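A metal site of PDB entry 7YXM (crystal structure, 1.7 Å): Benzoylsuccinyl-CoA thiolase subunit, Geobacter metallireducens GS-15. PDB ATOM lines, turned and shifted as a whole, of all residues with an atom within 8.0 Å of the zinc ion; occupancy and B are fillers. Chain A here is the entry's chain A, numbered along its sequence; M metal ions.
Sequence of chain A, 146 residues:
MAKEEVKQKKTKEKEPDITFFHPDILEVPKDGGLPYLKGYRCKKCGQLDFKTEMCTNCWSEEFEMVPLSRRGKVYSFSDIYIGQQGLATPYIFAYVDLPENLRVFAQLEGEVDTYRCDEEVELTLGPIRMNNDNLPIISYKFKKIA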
ATOM      1  N   ARG A  41      12.714   0.905 -19.324  1.00  0.00           N
ATOM      2  CA  ARG A  41      13.885   1.116 -20.173  1.00  0.00           C
ATOM      3  C   ARG A  41      13.573   2.131 -21.267  1.00  0.00           C
ATOM      4  O   ARG A  41      12.630   1.945 -22.044  1.00  0.00           O
ATOM      5  CB  ARG A  41      14.369  -0.183 -20.836  1.00  0.00           C
ATOM      6  CG  ARG A  41      15.699  -0.029 -21.628  1.00  0.00           C
ATOM      7  CD  ARG A  41      16.194  -1.387 -22.265  1.00  0.00           C
ATOM      8  NE  ARG A  41      16.299  -2.442 -21.261  1.00  0.00           N
ATOM      9  CZ  ARG A  41      17.346  -2.602 -20.439  1.00  0.00           C
ATOM     10  NH1 ARG A  41      18.392  -1.778 -20.525  1.00  0.00           N
ATOM     11  NH2 ARG A  41      17.332  -3.580 -19.548  1.00  0.00           N
ATOM     12  N   CYS A  42      14.418   3.162 -21.354  1.00  0.00           N
ATOM     13  CA  CYS A  42      14.318   4.133 -22.428  1.00  0.00           C
ATOM     14  C   CYS A  42      14.513   3.472 -23.789  1.00  0.00           C
ATOM     15  O   CYS A  42      15.511   2.790 -24.026  1.00  0.00           O
ATOM     16  CB  CYS A  42      15.374   5.240 -22.219  1.00  0.00           C
ATOM     17  SG  CYS A  42      15.361   6.390 -23.583  1.00  0.00           S
ATOM     18  N   LYS A  43      13.529   3.667 -24.670  1.00  0.00           N
ATOM     19  CA  LYS A  43      13.584   3.064 -25.997  1.00  0.00           C
ATOM     20  C   LYS A  43      14.562   3.759 -26.936  1.00  0.00           C
ATOM     21  O   LYS A  43      14.892   3.200 -27.983  1.00  0.00           O
ATOM     22  CB  LYS A  43      12.183   3.086 -26.613  1.00  0.00           C
ATOM     23  CG  LYS A  43      11.265   2.010 -26.031  1.00  0.00           C
ATOM     24  CD  LYS A  43       9.945   1.920 -26.828  1.00  0.00           C
ATOM     25  CE  LYS A  43       9.798   0.609 -27.616  1.00  0.00           C
ATOM     26  NZ  LYS A  43      10.383  -0.570 -26.899  1.00  0.00           N
ATOM     27  N   LYS A  44      15.036   4.944 -26.573  1.00  0.00           N
ATOM     28  CA  LYS A  44      15.971   5.664 -27.421  1.00  0.00           C
ATOM     29  C   LYS A  44      17.428   5.363 -27.070  1.00  0.00           C
ATOM     30  O   LYS A  44      18.251   5.151 -27.960  1.00  0.00           O
ATOM     31  CB  LYS A  44      15.720   7.176 -27.317  1.00  0.00           C
ATOM     32  CG  LYS A  44      16.549   7.969 -28.324  1.00  0.00           C
ATOM     33  CD  LYS A  44      16.879   9.366 -27.856  1.00  0.00           C
ATOM     34  CE  LYS A  44      16.238  10.431 -28.752  1.00  0.00           C
ATOM     35  NZ  LYS A  44      16.189  11.741 -28.052  1.00  0.00           N
ATOM     36  N   CYS A  45      17.782   5.397 -25.797  1.00  0.00           N
ATOM     37  CA  CYS A  45      19.163   5.249 -25.383  1.00  0.00           C
ATOM     38  C   CYS A  45      19.409   3.981 -24.592  1.00  0.00           C
ATOM     39  O   CYS A  45      20.571   3.572 -24.440  1.00  0.00           O
ATOM     40  CB  CYS A  45      19.576   6.475 -24.576  1.00  0.00           C
ATOM     41  SG  CYS A  45      19.126   6.449 -22.843  1.00  0.00           S
ATOM     42  N   GLY A  46      18.354   3.318 -24.171  1.00  0.00           N
ATOM     43  CA  GLY A  46      18.534   2.036 -23.522  1.00  0.00           C
ATOM     44  C   GLY A  46      18.728   2.130 -22.017  1.00  0.00           C
ATOM     45  O   GLY A  46      18.858   1.088 -21.371  1.00  0.00           O
ATOM     46  N   GLN A  47      18.710   3.331 -21.423  1.00  0.00           N
ATOM     47  CA  GLN A  47      18.906   3.426 -19.968  1.00  0.00           C
ATOM     48  C   GLN A  47      17.777   2.761 -19.200  1.00  0.00           C
ATOM     49  O   GLN A  47      16.598   3.147 -19.338  1.00  0.00           O
ATOM     50  CB  GLN A  47      19.002   4.891 -19.521  1.00  0.00           C
ATOM     51  CG  GLN A  47      19.186   5.022 -18.001  1.00  0.00           C
ATOM     52  CD  GLN A  47      19.675   6.412 -17.592  1.00  0.00           C
ATOM     53  OE1 GLN A  47      20.889   6.694 -17.584  1.00  0.00           O
ATOM     54  NE2 GLN A  47      18.762   7.281 -17.275  1.00  0.00           N
ATOM     55  N   LEU A  48      18.108   1.854 -18.284  1.00  0.00           N
ATOM     56  CA  LEU A  48      17.091   1.315 -17.362  1.00  0.00           C
ATOM     57  C   LEU A  48      16.990   2.171 -16.094  1.00  0.00           C
ATOM     58  O   LEU A  48      18.005   2.554 -15.514  1.00  0.00           O
ATOM     59  CB  LEU A  48      17.413  -0.115 -16.954  1.00  0.00           C
ATOM     60  CG  LEU A  48      16.382  -0.908 -16.156  1.00  0.00           C
ATOM     61  CD1 LEU A  48      15.083  -1.022 -16.952  1.00  0.00           C
ATOM     62  CD2 LEU A  48      16.956  -2.263 -15.807  1.00  0.00           C
ATOM     63  N   MET A  54      10.604  11.431 -17.838  1.00  0.00           N
ATOM     64  CA  MET A  54      11.486  11.496 -19.008  1.00  0.00           C
ATOM     65  C   MET A  54      12.830  10.871 -18.649  1.00  0.00           C
ATOM     66  O   MET A  54      13.211  10.915 -17.510  1.00  0.00           O
ATOM     67  CB  MET A  54      11.670  12.925 -19.524  1.00  0.00           C
ATOM     68  CG  MET A  54      12.258  13.868 -18.539  1.00  0.00           C
ATOM     69  SD  MET A  54      12.408  15.539 -19.191  1.00  0.00           S
ATOM     70  CE  MET A  54      11.098  15.614 -20.389  1.00  0.00           C
ATOM     71  N   CYS A  55      13.475  10.239 -19.611  1.00  0.00           N
ATOM     72  CA  CYS A  55      14.774   9.634 -19.400  1.00  0.00           C
ATOM     73  C   CYS A  55      15.792  10.687 -18.930  1.00  0.00           C
ATOM     74  O   CYS A  55      15.958  11.721 -19.573  1.00  0.00           O
ATOM     75  CB  CYS A  55      15.260   9.004 -20.688  1.00  0.00           C
ATOM     76  SG  CYS A  55      16.910   8.288 -20.549  1.00  0.00           S
ATOM     77  N   THR A  56      16.475  10.410 -17.816  1.00  0.00           N
ATOM     78  CA  THR A  56      17.386  11.419 -17.296  1.00  0.00           C
ATOM     79  C   THR A  56      18.670  11.473 -18.106  1.00  0.00           C
ATOM     80  O   THR A  56      19.448  12.427 -17.953  1.00  0.00           O
ATOM     81  CB  THR A  56      17.734  11.163 -15.820  1.00  0.00           C
ATOM     82  OG1 THR A  56      18.412   9.901 -15.747  1.00  0.00           O
ATOM     83  CG2 THR A  56      16.492  11.117 -14.952  1.00  0.00           C
ATOM     84  N   ASN A  57      18.909  10.494 -18.973  1.00  0.00           N
ATOM     85  CA  ASN A  57      20.080  10.537 -19.837  1.00  0.00           C
ATOM     86  C   ASN A  57      19.823  11.272 -21.143  1.00  0.00           C
ATOM     87  O   ASN A  57      20.682  12.024 -21.589  1.00  0.00           O
ATOM     88  CB  ASN A  57      20.553   9.114 -20.130  1.00  0.00           C
ATOM     89  CG  ASN A  57      21.781   9.089 -20.969  1.00  0.00           C
ATOM     90  OD1 ASN A  57      22.818   9.616 -20.571  1.00  0.00           O
ATOM     91  ND2 ASN A  57      21.690   8.502 -22.145  1.00  0.00           N
ATOM     92  N   CYS A  58      18.671  11.033 -21.810  1.00  0.00           N
ATOM     93  CA  CYS A  58      18.483  11.508 -23.178  1.00  0.00           C
ATOM     94  C   CYS A  58      17.179  12.290 -23.372  1.00  0.00           C
ATOM     95  O   CYS A  58      16.966  12.826 -24.459  1.00  0.00           O
ATOM     96  CB  CYS A  58      18.535  10.324 -24.174  1.00  0.00           C
ATOM     97  SG  CYS A  58      17.011   9.273 -24.181  1.00  0.00           S
ATOM     98  N   TRP A  59      16.339  12.357 -22.338  1.00  0.00           N
ATOM     99  CA  TRP A  59      15.082  13.111 -22.254  1.00  0.00           C
ATOM    100  C   TRP A  59      13.970  12.508 -23.098  1.00  0.00           C
ATOM    101  O   TRP A  59      12.871  13.071 -23.177  1.00  0.00           O
ATOM    102  CB  TRP A  59      15.275  14.588 -22.606  1.00  0.00           C
ATOM    103  CG  TRP A  59      15.888  15.404 -21.505  1.00  0.00           C
ATOM    104  CD1 TRP A  59      16.345  14.979 -20.303  1.00  0.00           C
ATOM    105  CD2 TRP A  59      16.100  16.808 -21.543  1.00  0.00           C
ATOM    106  NE1 TRP A  59      16.815  16.056 -19.569  1.00  0.00           N
ATOM    107  CE2 TRP A  59      16.669  17.193 -20.315  1.00  0.00           C
ATOM    108  CE3 TRP A  59      15.846  17.788 -22.500  1.00  0.00           C
ATOM    109  CZ2 TRP A  59      17.001  18.518 -20.031  1.00  0.00           C
ATOM    110  CZ3 TRP A  59      16.159  19.070 -22.225  1.00  0.00           C
ATOM    111  CH2 TRP A  59      16.738  19.439 -21.001  1.00  0.00           C
ATOM    112  N   SER A  60      14.198  11.343 -23.668  1.00  0.00           N
ATOM    113  CA  SER A  60      13.092  10.612 -24.291  1.00  0.00           C
ATOM    114  C   SER A  60      11.991  10.308 -23.278  1.00  0.00           C
ATOM    115  O   SER A  60      12.220  10.142 -22.066  1.00  0.00           O
ATOM    116  CB  SER A  60      13.616   9.310 -24.904  1.00  0.00           C
ATOM    117  OG  SER A  60      12.534   8.510 -25.366  1.00  0.00           O
ATOM    118  N   GLU A  61      10.767  10.236 -23.779  1.00  0.00           N
ATOM    119  CA  GLU A  61       9.622   9.864 -22.978  1.00  0.00           C
ATOM    120  C   GLU A  61       9.047   8.525 -23.400  1.00  0.00           C
ATOM    121  O   GLU A  61       7.906   8.191 -23.008  1.00  0.00           O
ATOM    122  CB  GLU A  61       8.536  10.946 -23.086  1.00  0.00           C
ATOM    123  CG  GLU A  61       9.007  12.365 -22.699  1.00  0.00           C
ATOM    124  CD  GLU A  61       7.863  13.371 -22.756  1.00  0.00           C
ATOM    125  OE1 GLU A  61       7.489  13.764 -23.883  1.00  0.00           O
ATOM    126  OE2 GLU A  61       7.331  13.728 -21.691  1.00  0.00           O
ATOM    127  N   GLU A  62       9.773   7.768 -24.183  1.00  0.00           N
ATOM    128  CA  GLU A  62       9.272   6.506 -24.725  1.00  0.00           C
ATOM    129  C   GLU A  62       9.965   5.350 -24.017  1.00  0.00           C
ATOM    130  O   GLU A  62      11.188   5.247 -24.061  1.00  0.00           O
ATOM    131  CB  GLU A  62       9.514   6.456 -26.241  1.00  0.00           C
ATOM    132  CG  GLU A  62       8.278   6.363 -27.090  1.00  0.00           C
ATOM    133  CD  GLU A  62       8.595   5.954 -28.521  1.00  0.00           C
ATOM    134  OE1 GLU A  62       9.279   6.720 -29.229  1.00  0.00           O
ATOM    135  OE2 GLU A  62       8.168   4.851 -28.940  1.00  0.00           O
ATOM    136  N   PHE A  63       9.185   4.498 -23.353  1.00  0.00           N
ATOM    137  CA  PHE A  63       9.750   3.442 -22.514  1.00  0.00           C
ATOM    138  C   PHE A  63       9.128   2.076 -22.772  1.00  0.00           C
ATOM    139  O   PHE A  63       8.035   1.946 -23.326  1.00  0.00           O
ATOM    140  CB  PHE A  63       9.522   3.758 -21.025  1.00  0.00           C
ATOM    141  CG  PHE A  63      10.170   5.040 -20.587  1.00  0.00           C
ATOM    142  CD1 PHE A  63      11.494   5.052 -20.199  1.00  0.00           C
ATOM    143  CD2 PHE A  63       9.459   6.231 -20.577  1.00  0.00           C
ATOM    144  CE1 PHE A  63      12.106   6.229 -19.790  1.00  0.00           C
ATOM    145  CE2 PHE A  63      10.079   7.411 -20.161  1.00  0.00           C
ATOM    146  CZ  PHE A  63      11.400   7.399 -19.776  1.00  0.00           C
HETATM  147 ZN    ZN M   1      17.201   7.676 -22.821  1.00  0.00          ZN
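The side-chain sulfur (SG) of Cys 58 is bound to the zinc ion (2.1 Å).
SG of Cys 45 binds the zinc ion, 2.3 Å away.
The side-chain sulfur (SG) of Cys 42 is bound to the zinc ion (2.4 Å).
The zinc ion is bound by the side-chain sulfur (SG) of Cys 55, 2.4 Å away.
The backbone NH (N) of Cys 55 lies within hydrogen-bond range of the backbone carbonyl oxygen (O) of Ser 60 (2.8 Å).
The side-chain sulfur of Cys 58 sits close to the backbone NH of Ser 60, 3.5 Å away.
The backbone NH of Cys 42 sits at hydrogen-bond distance from the backbone carbonyl oxygen of Gln 47.
The side-chain sulfur (SG) of Cys 42 lies close to the backbone NH (N) of Lys 44 (3.3 Å).
The backbone NH of Gln 47 lies close to the side-chain sulfur of Cys 45, 3.5 Å away.
SG of Cys 55 sits close to N of Asn 57.
The side-chain sulfur (SG) of Cys 45 sits close to the side-chain amide nitrogen (ND2) of Asn 57 (3.4 Å).
Of the 18 residues printed, 4 come within 4 Å of the zinc ion.
Along chain A the residues within 4 Å of the zinc ion span positions 42 to 58.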
